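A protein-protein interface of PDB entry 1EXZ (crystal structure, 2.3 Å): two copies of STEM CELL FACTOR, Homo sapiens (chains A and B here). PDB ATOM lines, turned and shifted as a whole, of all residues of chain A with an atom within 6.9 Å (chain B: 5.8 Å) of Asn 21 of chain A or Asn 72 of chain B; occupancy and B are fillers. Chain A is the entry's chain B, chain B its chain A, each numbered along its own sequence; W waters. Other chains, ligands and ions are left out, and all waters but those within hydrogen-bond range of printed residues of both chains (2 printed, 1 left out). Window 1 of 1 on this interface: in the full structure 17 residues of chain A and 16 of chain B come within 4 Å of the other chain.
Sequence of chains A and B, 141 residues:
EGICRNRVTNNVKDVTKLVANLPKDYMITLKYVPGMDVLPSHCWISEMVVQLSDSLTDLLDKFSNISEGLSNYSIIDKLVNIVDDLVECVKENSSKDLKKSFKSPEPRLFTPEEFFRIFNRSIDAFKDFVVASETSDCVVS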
ATOM      1  N   VAL A  15      13.240  -7.506 -16.059  1.00  0.00           N
ATOM      2  CA  VAL A  15      13.862  -7.789 -14.779  1.00  0.00           C
ATOM      3  C   VAL A  15      14.940  -8.867 -14.874  1.00  0.00           C
ATOM      4  O   VAL A  15      16.048  -8.683 -14.371  1.00  0.00           O
ATOM      5  CB  VAL A  15      12.810  -8.207 -13.742  1.00  0.00           C
ATOM      6  CG1 VAL A  15      13.477  -8.530 -12.413  1.00  0.00           C
ATOM      7  CG2 VAL A  15      11.812  -7.084 -13.556  1.00  0.00           C
ATOM      8  N   THR A  16      14.633  -9.983 -15.531  1.00  0.00           N
ATOM      9  CA  THR A  16      15.610 -11.059 -15.648  1.00  0.00           C
ATOM     10  C   THR A  16      16.827 -10.564 -16.414  1.00  0.00           C
ATOM     11  O   THR A  16      17.967 -10.850 -16.043  1.00  0.00           O
ATOM     12  CB  THR A  16      15.027 -12.310 -16.375  1.00  0.00           C
ATOM     13  OG1 THR A  16      15.074 -12.116 -17.790  1.00  0.00           O
ATOM     14  CG2 THR A  16      13.588 -12.546 -15.960  1.00  0.00           C
ATOM     15  N   LYS A  17      16.577  -9.812 -17.480  1.00  0.00           N
ATOM     16  CA  LYS A  17      17.652  -9.265 -18.296  1.00  0.00           C
ATOM     17  C   LYS A  17      18.593  -8.390 -17.468  1.00  0.00           C
ATOM     18  O   LYS A  17      19.807  -8.416 -17.666  1.00  0.00           O
ATOM     19  CB  LYS A  17      17.073  -8.438 -19.447  1.00  0.00           C
ATOM     20  CG  LYS A  17      16.379  -9.270 -20.504  1.00  0.00           C
ATOM     21  CD  LYS A  17      15.927  -8.414 -21.683  1.00  0.00           C
ATOM     22  CE  LYS A  17      15.259  -9.272 -22.751  1.00  0.00           C
ATOM     23  NZ  LYS A  17      14.891  -8.470 -23.951  1.00  0.00           N
ATOM     24  N   LEU A  18      18.021  -7.616 -16.547  1.00  0.00           N
ATOM     25  CA  LEU A  18      18.801  -6.729 -15.685  1.00  0.00           C
ATOM     26  C   LEU A  18      19.622  -7.533 -14.693  1.00  0.00           C
ATOM     27  O   LEU A  18      20.802  -7.261 -14.496  1.00  0.00           O
ATOM     28  CB  LEU A  18      17.882  -5.778 -14.916  1.00  0.00           C
ATOM     29  CG  LEU A  18      18.518  -4.786 -13.946  1.00  0.00           C
ATOM     30  CD1 LEU A  18      19.429  -3.847 -14.695  1.00  0.00           C
ATOM     31  CD2 LEU A  18      17.417  -4.001 -13.237  1.00  0.00           C
ATOM     32  N   VAL A  19      18.995  -8.514 -14.054  1.00  0.00           N
ATOM     33  CA  VAL A  19      19.718  -9.342 -13.103  1.00  0.00           C
ATOM     34  C   VAL A  19      20.900  -9.985 -13.848  1.00  0.00           C
ATOM     35  O   VAL A  19      22.004 -10.085 -13.318  1.00  0.00           O
ATOM     36  CB  VAL A  19      18.789 -10.420 -12.508  1.00  0.00           C
ATOM     37  CG1 VAL A  19      19.572 -11.353 -11.577  1.00  0.00           C
ATOM     38  CG2 VAL A  19      17.656  -9.745 -11.744  1.00  0.00           C
ATOM     39  N   ALA A  20      20.654 -10.389 -15.090  1.00  0.00           N
ATOM     40  CA  ALA A  20      21.673 -10.999 -15.945  1.00  0.00           C
ATOM     41  C   ALA A  20      22.772  -9.999 -16.315  1.00  0.00           C
ATOM     42  O   ALA A  20      23.904 -10.383 -16.636  1.00  0.00           O
ATOM     43  CB  ALA A  20      21.021 -11.521 -17.224  1.00  0.00           C
ATOM     44  N   ASN A  21      22.433  -8.715 -16.276  1.00  0.00           N
ATOM     45  CA  ASN A  21      23.392  -7.683 -16.639  1.00  0.00           C
ATOM     46  C   ASN A  21      23.982  -6.981 -15.420  1.00  0.00           C
ATOM     47  O   ASN A  21      24.668  -5.970 -15.536  1.00  0.00           O
ATOM     48  CB  ASN A  21      22.725  -6.674 -17.556  1.00  0.00           C
ATOM     49  CG  ASN A  21      23.673  -6.110 -18.556  1.00  0.00           C
ATOM     50  OD1 ASN A  21      24.366  -6.856 -19.246  1.00  0.00           O
ATOM     51  ND2 ASN A  21      23.720  -4.786 -18.654  1.00  0.00           N
ATOM     52  N   LEU A  22      23.699  -7.541 -14.254  1.00  0.00           N
ATOM     53  CA  LEU A  22      24.192  -7.023 -12.995  1.00  0.00           C
ATOM     54  C   LEU A  22      25.098  -8.098 -12.402  1.00  0.00           C
ATOM     55  O   LEU A  22      24.758  -9.285 -12.407  1.00  0.00           O
ATOM     56  CB  LEU A  22      23.019  -6.761 -12.055  1.00  0.00           C
ATOM     57  CG  LEU A  22      22.646  -5.356 -11.572  1.00  0.00           C
ATOM     58  CD1 LEU A  22      23.117  -4.252 -12.520  1.00  0.00           C
ATOM     59  CD2 LEU A  22      21.139  -5.345 -11.413  1.00  0.00           C
ATOM     60  N   PRO A  23      26.278  -7.710 -11.911  1.00  0.00           N
ATOM     61  CA  PRO A  23      27.154  -8.730 -11.330  1.00  0.00           C
ATOM     62  C   PRO A  23      26.472  -9.411 -10.138  1.00  0.00           C
ATOM     63  O   PRO A  23      25.897  -8.737  -9.271  1.00  0.00           O
ATOM     64  CB  PRO A  23      28.402  -7.936 -10.931  1.00  0.00           C
ATOM     65  CG  PRO A  23      27.890  -6.512 -10.764  1.00  0.00           C
ATOM     66  CD  PRO A  23      26.900  -6.374 -11.879  1.00  0.00           C
ATOM     67  N   PHE A  63      24.649   4.341 -12.933  1.00  0.00           N
ATOM     68  CA  PHE A  63      24.772   3.981 -14.337  1.00  0.00           C
ATOM     69  C   PHE A  63      24.728   5.191 -15.253  1.00  0.00           C
ATOM     70  O   PHE A  63      24.369   6.291 -14.827  1.00  0.00           O
ATOM     71  CB  PHE A  63      23.681   2.982 -14.731  1.00  0.00           C
ATOM     72  CG  PHE A  63      23.685   1.724 -13.902  1.00  0.00           C
ATOM     73  CD1 PHE A  63      22.948   1.649 -12.723  1.00  0.00           C
ATOM     74  CD2 PHE A  63      24.474   0.633 -14.271  1.00  0.00           C
ATOM     75  CE1 PHE A  63      22.999   0.505 -11.919  1.00  0.00           C
ATOM     76  CE2 PHE A  63      24.535  -0.513 -13.478  1.00  0.00           C
ATOM     77  CZ  PHE A  63      23.799  -0.580 -12.300  1.00  0.00           C
ATOM     78  N   LEU A  70      20.947  -2.576 -25.256  1.00  0.00           N
ATOM     79  CA  LEU A  70      20.806  -2.995 -23.863  1.00  0.00           C
ATOM     80  C   LEU A  70      21.366  -1.962 -22.881  1.00  0.00           C
ATOM     81  O   LEU A  70      22.587  -1.780 -22.784  1.00  0.00           O
ATOM     82  CB  LEU A  70      21.518  -4.338 -23.648  1.00  0.00           C
ATOM     83  CG  LEU A  70      21.072  -5.219 -22.468  1.00  0.00           C
ATOM     84  CD1 LEU A  70      22.085  -6.353 -22.286  1.00  0.00           C
ATOM     85  CD2 LEU A  70      20.958  -4.398 -21.180  1.00  0.00           C
ATOM     86  N   SER A  71      20.475  -1.307 -22.137  1.00  0.00           N
ATOM     87  CA  SER A  71      20.893  -0.298 -21.165  1.00  0.00           C
ATOM     88  C   SER A  71      20.351  -0.569 -19.774  1.00  0.00           C
ATOM     89  O   SER A  71      19.141  -0.652 -19.583  1.00  0.00           O
ATOM     90  CB  SER A  71      20.428   1.089 -21.613  1.00  0.00           C
ATOM     91  OG  SER A  71      20.793   2.076 -20.661  1.00  0.00           O
ATOM     92  N   ASN A  72      21.238  -0.700 -18.794  1.00  0.00           N
ATOM     93  CA  ASN A  72      20.782  -0.933 -17.430  1.00  0.00           C
ATOM     94  C   ASN A  72      20.065   0.303 -16.880  1.00  0.00           C
ATOM     95  O   ASN A  72      19.095   0.175 -16.127  1.00  0.00           O
ATOM     96  CB  ASN A  72      21.948  -1.321 -16.513  1.00  0.00           C
ATOM     97  CG  ASN A  72      22.369  -2.792 -16.673  1.00  0.00           C
ATOM     98  OD1 ASN A  72      21.651  -3.599 -17.270  1.00  0.00           O
ATOM     99  ND2 ASN A  72      23.533  -3.139 -16.125  1.00  0.00           N
ATOM    100  N   ILE A  75      16.424   0.229 -18.188  1.00  0.00           N
ATOM    101  CA  ILE A  75      15.570  -0.755 -17.545  1.00  0.00           C
ATOM    102  C   ILE A  75      15.186  -0.326 -16.135  1.00  0.00           C
ATOM    103  O   ILE A  75      14.029  -0.458 -15.737  1.00  0.00           O
ATOM    104  CB  ILE A  75      16.269  -2.124 -17.524  1.00  0.00           C
ATOM    105  CG1 ILE A  75      16.378  -2.634 -18.972  1.00  0.00           C
ATOM    106  CG2 ILE A  75      15.499  -3.119 -16.649  1.00  0.00           C
ATOM    107  CD1 ILE A  75      17.245  -3.877 -19.131  1.00  0.00           C
ATOM    108  N   LYS B  17      30.893   1.239 -23.487  1.00  0.00           N
ATOM    109  CA  LYS B  17      29.563   0.700 -23.261  1.00  0.00           C
ATOM    110  C   LYS B  17      29.572  -0.109 -21.961  1.00  0.00           C
ATOM    111  O   LYS B  17      28.715   0.086 -21.094  1.00  0.00           O
ATOM    112  CB  LYS B  17      29.141  -0.193 -24.431  1.00  0.00           C
ATOM    113  CG  LYS B  17      27.659  -0.584 -24.413  1.00  0.00           C
ATOM    114  CD  LYS B  17      27.289  -1.454 -25.613  1.00  0.00           C
ATOM    115  CE  LYS B  17      25.775  -1.676 -25.712  1.00  0.00           C
ATOM    116  NZ  LYS B  17      25.182  -2.399 -24.539  1.00  0.00           N
ATOM    117  N   LEU B  18      30.557  -0.995 -21.817  1.00  0.00           N
ATOM    118  CA  LEU B  18      30.668  -1.827 -20.610  1.00  0.00           C
ATOM    119  C   LEU B  18      30.668  -0.964 -19.352  1.00  0.00           C
ATOM    120  O   LEU B  18      29.915  -1.214 -18.418  1.00  0.00           O
ATOM    121  CB  LEU B  18      31.956  -2.645 -20.634  1.00  0.00           C
ATOM    122  CG  LEU B  18      31.910  -4.030 -19.995  1.00  0.00           C
ATOM    123  CD1 LEU B  18      33.335  -4.512 -19.822  1.00  0.00           C
ATOM    124  CD2 LEU B  18      31.174  -4.017 -18.679  1.00  0.00           C
ATOM    125  N   ASN B  21      27.469   0.405 -18.268  1.00  0.00           N
ATOM    126  CA  ASN B  21      26.559  -0.563 -17.674  1.00  0.00           C
ATOM    127  C   ASN B  21      27.040  -1.332 -16.457  1.00  0.00           C
ATOM    128  O   ASN B  21      26.406  -2.303 -16.040  1.00  0.00           O
ATOM    129  CB  ASN B  21      26.074  -1.523 -18.752  1.00  0.00           C
ATOM    130  CG  ASN B  21      25.025  -0.892 -19.629  1.00  0.00           C
ATOM    131  OD1 ASN B  21      23.855  -0.794 -19.239  1.00  0.00           O
ATOM    132  ND2 ASN B  21      25.438  -0.417 -20.806  1.00  0.00           N
ATOM    133  N   LEU B  22      28.160  -0.906 -15.889  1.00  0.00           N
ATOM    134  CA  LEU B  22      28.675  -1.524 -14.671  1.00  0.00           C
ATOM    135  C   LEU B  22      28.471  -0.492 -13.573  1.00  0.00           C
ATOM    136  O   LEU B  22      28.803   0.666 -13.750  1.00  0.00           O
ATOM    137  CB  LEU B  22      30.160  -1.847 -14.793  1.00  0.00           C
ATOM    138  CG  LEU B  22      30.556  -3.071 -15.615  1.00  0.00           C
ATOM    139  CD1 LEU B  22      32.072  -3.164 -15.648  1.00  0.00           C
ATOM    140  CD2 LEU B  22      29.940  -4.342 -15.008  1.00  0.00           C
ATOM    141  N   LEU B  60      33.841 -12.217 -15.751  1.00  0.00           N
ATOM    142  CA  LEU B  60      32.958 -12.856 -16.709  1.00  0.00           C
ATOM    143  C   LEU B  60      31.986 -13.846 -16.064  1.00  0.00           C
ATOM    144  O   LEU B  60      30.836 -13.967 -16.487  1.00  0.00           O
ATOM    145  CB  LEU B  60      33.800 -13.562 -17.771  1.00  0.00           C
ATOM    146  CG  LEU B  60      33.055 -14.274 -18.902  1.00  0.00           C
ATOM    147  CD1 LEU B  60      32.103 -13.307 -19.596  1.00  0.00           C
ATOM    148  CD2 LEU B  60      34.076 -14.825 -19.892  1.00  0.00           C
ATOM    149  N   PHE B  63      28.389 -12.583 -14.689  1.00  0.00           N
ATOM    150  CA  PHE B  63      27.268 -12.192 -15.539  1.00  0.00           C
ATOM    151  C   PHE B  63      26.715 -13.393 -16.304  1.00  0.00           C
ATOM    152  O   PHE B  63      27.435 -14.351 -16.580  1.00  0.00           O
ATOM    153  CB  PHE B  63      27.701 -11.104 -16.537  1.00  0.00           C
ATOM    154  CG  PHE B  63      28.181  -9.835 -15.887  1.00  0.00           C
ATOM    155  CD1 PHE B  63      29.453  -9.757 -15.331  1.00  0.00           C
ATOM    156  CD2 PHE B  63      27.349  -8.723 -15.804  1.00  0.00           C
ATOM    157  CE1 PHE B  63      29.893  -8.591 -14.703  1.00  0.00           C
ATOM    158  CE2 PHE B  63      27.778  -7.552 -15.178  1.00  0.00           C
ATOM    159  CZ  PHE B  63      29.053  -7.489 -14.626  1.00  0.00           C
ATOM    160  N   SER B  64      25.431 -13.339 -16.642  1.00  0.00           N
ATOM    161  CA  SER B  64      24.792 -14.413 -17.387  1.00  0.00           C
ATOM    162  C   SER B  64      24.728 -14.022 -18.856  1.00  0.00           C
ATOM    163  O   SER B  64      24.729 -12.840 -19.193  1.00  0.00           O
ATOM    164  CB  SER B  64      23.391 -14.670 -16.846  1.00  0.00           C
ATOM    165  OG  SER B  64      23.447 -15.024 -15.474  1.00  0.00           O
ATOM    166  N   ILE B  66      23.425 -13.603 -22.891  1.00  0.00           N
ATOM    167  CA  ILE B  66      22.333 -12.975 -23.654  1.00  0.00           C
ATOM    168  C   ILE B  66      22.991 -12.154 -24.774  1.00  0.00           C
ATOM    169  O   ILE B  66      22.512 -11.082 -25.156  1.00  0.00           O
ATOM    170  CB  ILE B  66      21.446 -12.021 -22.797  1.00  0.00           C
ATOM    171  CG1 ILE B  66      22.301 -11.295 -21.754  1.00  0.00           C
ATOM    172  CG2 ILE B  66      20.295 -12.796 -22.174  1.00  0.00           C
ATOM    173  CD1 ILE B  66      21.520 -10.310 -20.900  1.00  0.00           C
ATOM    174  N   LEU B  70      24.693  -6.914 -27.313  1.00  0.00           N
ATOM    175  CA  LEU B  70      25.798  -6.298 -26.567  1.00  0.00           C
ATOM    176  C   LEU B  70      25.616  -6.285 -25.050  1.00  0.00           C
ATOM    177  O   LEU B  70      25.580  -5.221 -24.431  1.00  0.00           O
ATOM    178  CB  LEU B  70      26.027  -4.863 -27.045  1.00  0.00           C
ATOM    179  CG  LEU B  70      26.603  -4.629 -28.440  1.00  0.00           C
ATOM    180  CD1 LEU B  70      26.508  -3.148 -28.781  1.00  0.00           C
ATOM    181  CD2 LEU B  70      28.044  -5.111 -28.491  1.00  0.00           C
ATOM    182  N   SER B  71      25.500  -7.465 -24.452  1.00  0.00           N
ATOM    183  CA  SER B  71      25.349  -7.574 -23.005  1.00  0.00           C
ATOM    184  C   SER B  71      26.732  -7.461 -22.360  1.00  0.00           C
ATOM    185  O   SER B  71      27.748  -7.557 -23.040  1.00  0.00           O
ATOM    186  CB  SER B  71      24.732  -8.926 -22.644  1.00  0.00           C
ATOM    187  OG  SER B  71      25.567  -9.987 -23.077  1.00  0.00           O
ATOM    188  N   ASN B  72      26.772  -7.261 -21.048  1.00  0.00           N
ATOM    189  CA  ASN B  72      28.049  -7.165 -20.361  1.00  0.00           C
ATOM    190  C   ASN B  72      28.820  -8.455 -20.590  1.00  0.00           C
ATOM    191  O   ASN B  72      30.005  -8.431 -20.923  1.00  0.00           O
ATOM    192  CB  ASN B  72      27.845  -6.913 -18.857  1.00  0.00           C
ATOM    193  CG  ASN B  72      27.355  -5.498 -18.568  1.00  0.00           C
ATOM    194  OD1 ASN B  72      27.551  -4.599 -19.377  1.00  0.00           O
ATOM    195  ND2 ASN B  72      26.731  -5.294 -17.408  1.00  0.00           N
ATOM    196  N   TYR B  73      28.135  -9.579 -20.439  1.00  0.00           N
ATOM    197  CA  TYR B  73      28.750 -10.887 -20.634  1.00  0.00           C
ATOM    198  C   TYR B  73      29.501 -10.962 -21.965  1.00  0.00           C
ATOM    199  O   TYR B  73      30.678 -11.331 -22.020  1.00  0.00           O
ATOM    200  CB  TYR B  73      27.679 -11.990 -20.609  1.00  0.00           C
ATOM    201  CG  TYR B  73      28.263 -13.389 -20.695  1.00  0.00           C
ATOM    202  CD1 TYR B  73      28.541 -14.122 -19.544  1.00  0.00           C
ATOM    203  CD2 TYR B  73      28.611 -13.941 -21.925  1.00  0.00           C
ATOM    204  CE1 TYR B  73      29.158 -15.371 -19.619  1.00  0.00           C
ATOM    205  CE2 TYR B  73      29.230 -15.182 -22.012  1.00  0.00           C
ATOM    206  CZ  TYR B  73      29.502 -15.892 -20.861  1.00  0.00           C
ATOM    207  OH  TYR B  73      30.133 -17.115 -20.951  1.00  0.00           O
ATOM    208  N   SER B  74      28.806 -10.609 -23.038  1.00  0.00           N
ATOM    209  CA  SER B  74      29.374 -10.657 -24.378  1.00  0.00           C
ATOM    210  C   SER B  74      30.577  -9.749 -24.582  1.00  0.00           C
ATOM    211  O   SER B  74      31.586 -10.158 -25.163  1.00  0.00           O
ATOM    212  CB  SER B  74      28.285 -10.321 -25.402  1.00  0.00           C
ATOM    213  OG  SER B  74      27.543  -9.185 -24.982  1.00  0.00           O
ATOM    214  N   ILE B  75      30.470  -8.513 -24.113  1.00  0.00           N
ATOM    215  CA  ILE B  75      31.556  -7.556 -24.258  1.00  0.00           C
ATOM    216  C   ILE B  75      32.798  -8.020 -23.488  1.00  0.00           C
ATOM    217  O   ILE B  75      33.917  -7.964 -23.998  1.00  0.00           O
ATOM    218  CB  ILE B  75      31.107  -6.168 -23.758  1.00  0.00           C
ATOM    219  CG1 ILE B  75      30.040  -5.612 -24.708  1.00  0.00           C
ATOM    220  CG2 ILE B  75      32.306  -5.224 -23.656  1.00  0.00           C
ATOM    221  CD1 ILE B  75      29.407  -4.324 -24.235  1.00  0.00           C
ATOM    222  N   ILE B  76      32.588  -8.473 -22.260  1.00  0.00           N
ATOM    223  CA  ILE B  76      33.669  -8.954 -21.423  1.00  0.00           C
ATOM    224  C   ILE B  76      34.328 -10.154 -22.096  1.00  0.00           C
ATOM    225  O   ILE B  76      35.561 -10.220 -22.209  1.00  0.00           O
ATOM    226  CB  ILE B  76      33.132  -9.362 -20.048  1.00  0.00           C
ATOM    227  CG1 ILE B  76      32.510  -8.138 -19.366  1.00  0.00           C
ATOM    228  CG2 ILE B  76      34.257  -9.941 -19.199  1.00  0.00           C
ATOM    229  CD1 ILE B  76      31.834  -8.443 -18.042  1.00  0.00           C
ATOM    230  N   ASP B  77      33.509 -11.098 -22.554  1.00  0.00           N
ATOM    231  CA  ASP B  77      34.040 -12.279 -23.239  1.00  0.00           C
ATOM    232  C   ASP B  77      34.920 -11.790 -24.390  1.00  0.00           C
ATOM    233  O   ASP B  77      36.008 -12.309 -24.619  1.00  0.00           O
ATOM    234  CB  ASP B  77      32.898 -13.147 -23.782  1.00  0.00           C
ATOM    235  CG  ASP B  77      33.369 -14.525 -24.233  1.00  0.00           C
ATOM    236  OD1 ASP B  77      33.128 -14.878 -25.410  1.00  0.00           O
ATOM    237  OD2 ASP B  77      33.972 -15.258 -23.413  1.00  0.00           O
HETATM  238  O   HOH W   1      26.100  -4.281 -14.036  1.00  0.00           O
HETATM  239  O   HOH W   2      23.005   1.990 -18.885  1.00  0.00           O
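Water W1 bridges O of Asn 21 of chain A (2.7 Å) and O of Asn 21 of chain B (2.8 Å).
Water W2 lies within hydrogen-bond range of OG of Ser 71 of chain A, OD1 of Asn 21 of chain B and N of Asn 72 of chain A.
Asn 21 of chain A touches Ser 71 of chain B, and with the chains exchanged Ser 71 of chain A touches Asn 21 of chain B.
Asn 21 of chain A touches Asn 72 of chain B, and with the chains exchanged Asn 72 of chain A touches Asn 21 of chain B.
Leu 70 of chain A touches Asn 21 of chain B, but with the chains exchanged Asn 21 of chain A does not touch Leu 70 of chain B (5.6 Å).
Leu 70 of chain A touches Ser 71 of chain B, but with the chains exchanged Ser 71 of chain A does not touch Leu 70 of chain B (6.8 Å).
Positions printed for both chains: 17, 18, 21, 22, 63, 70, 71, 72 and 75.
Of the 15 pairs that touch across the chains among the printed residues, 8 have their exchanged pair printed and touching as well.
O of Lys 17 of chain B is in hydrogen-bond range of ND2 of Asn 21 of chain B, at 3.3 Å.
O of Leu 70 of chain B sits at hydrogen-bond distance from NZ of Lys 17 of chain B, at 2.9 Å.
ND2 of Asn 72 of chain B lies within hydrogen-bond range of O of Asn 21 of chain B (3.3 Å).
The backbone carbonyl oxygen of Ser 71 of chain B sits at hydrogen-bond distance from the side-chain hydroxyl of Ser 74 of chain B, 2.5 Å away.
ND2 of Asn 21 of chain A lies within hydrogen-bond range of OD1 of Asn 72 of chain A (2.8 Å).
Of the 14 printed residues of chain A, 8 touch a printed residue of chain B.
Hydrophobic or aromatic side chains of chain A that line the printed part of chain B: Ala 20, Pro 23, Phe 63 and Leu 70.
Of the 16 printed residues of chain B, 8 touch a printed residue of chain A.
Hydrophobic or aromatic side chains of chain B that line the printed part of chain A: Phe 63 and Ile 66.
Among the printed residues, 15 pairs touch across the chains.
Phe 63 of chain B touches Ala 20 of chain A.
CB of Ala 20 of chain A touches CD1 of Ile 66 of chain B (3.9 Å).
CE2 of Phe 63 of chain B touches O of Asn 21 of chain A, at 3.5 Å.
Asn 21 of chain A touches Ser 71 of chain B.
Phe 63 of chain B touches Leu 22 of chain A.
CE2 of Phe 63 of chain B touches N of Pro 23 of chain A (3.6 Å).
O of Asn 21 of chain B touches CE2 of Phe 63 of chain A, at 3.6 Å.
Phe 63 of chain A touches Leu 22 of chain B (CE2 to C, 3.9 Å).
O of Leu 70 of chain A touches ND2 of Asn 21 of chain B, at 3.7 Å.
Asn 21 of chain B touches Ser 71 of chain A (OD1 to C, 3.6 Å).
The side-chain amino group of Lys 17 of chain B lies within hydrogen-bond range of the backbone carbonyl oxygen of Leu 70 of chain A (3.2 Å).
The backbone NH (N) of Asn 72 of chain A is in hydrogen-bond range of the side-chain amide oxygen (OD1) of Asn 21 of chain B.
N of Ser 64 of chain B sits at hydrogen-bond distance from O of Ala 20 of chain A, 3.3 Å away.
The backbone carbonyl oxygen of Asn 21 of chain A is in hydrogen-bond range of the side-chain amide nitrogen of Asn 72 of chain B.
Lys 17 of chain A touches none of the printed residues of chain B.
Of chain B, only Phe 63 (3.5 Å), Ser 71 (3.95 Å) and Asn 72 (2.9 Å) come within 4 Å of Asn 21 of chain A.
Of the printed residues of chain B, Phe 63 of chain A touches Asn 21 (3.6 Å) and Leu 22 (3.9 Å).
Of the printed residues of chain B, Asn 72 of chain A touches Asn 21.
Printed residues of chain A within 4 Å of Lys 17 of chain B: Leu 70.
The nearest residue of chain B that does not touch Asn 21 of chain A is Asn 21 of chain B (4.02 Å).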
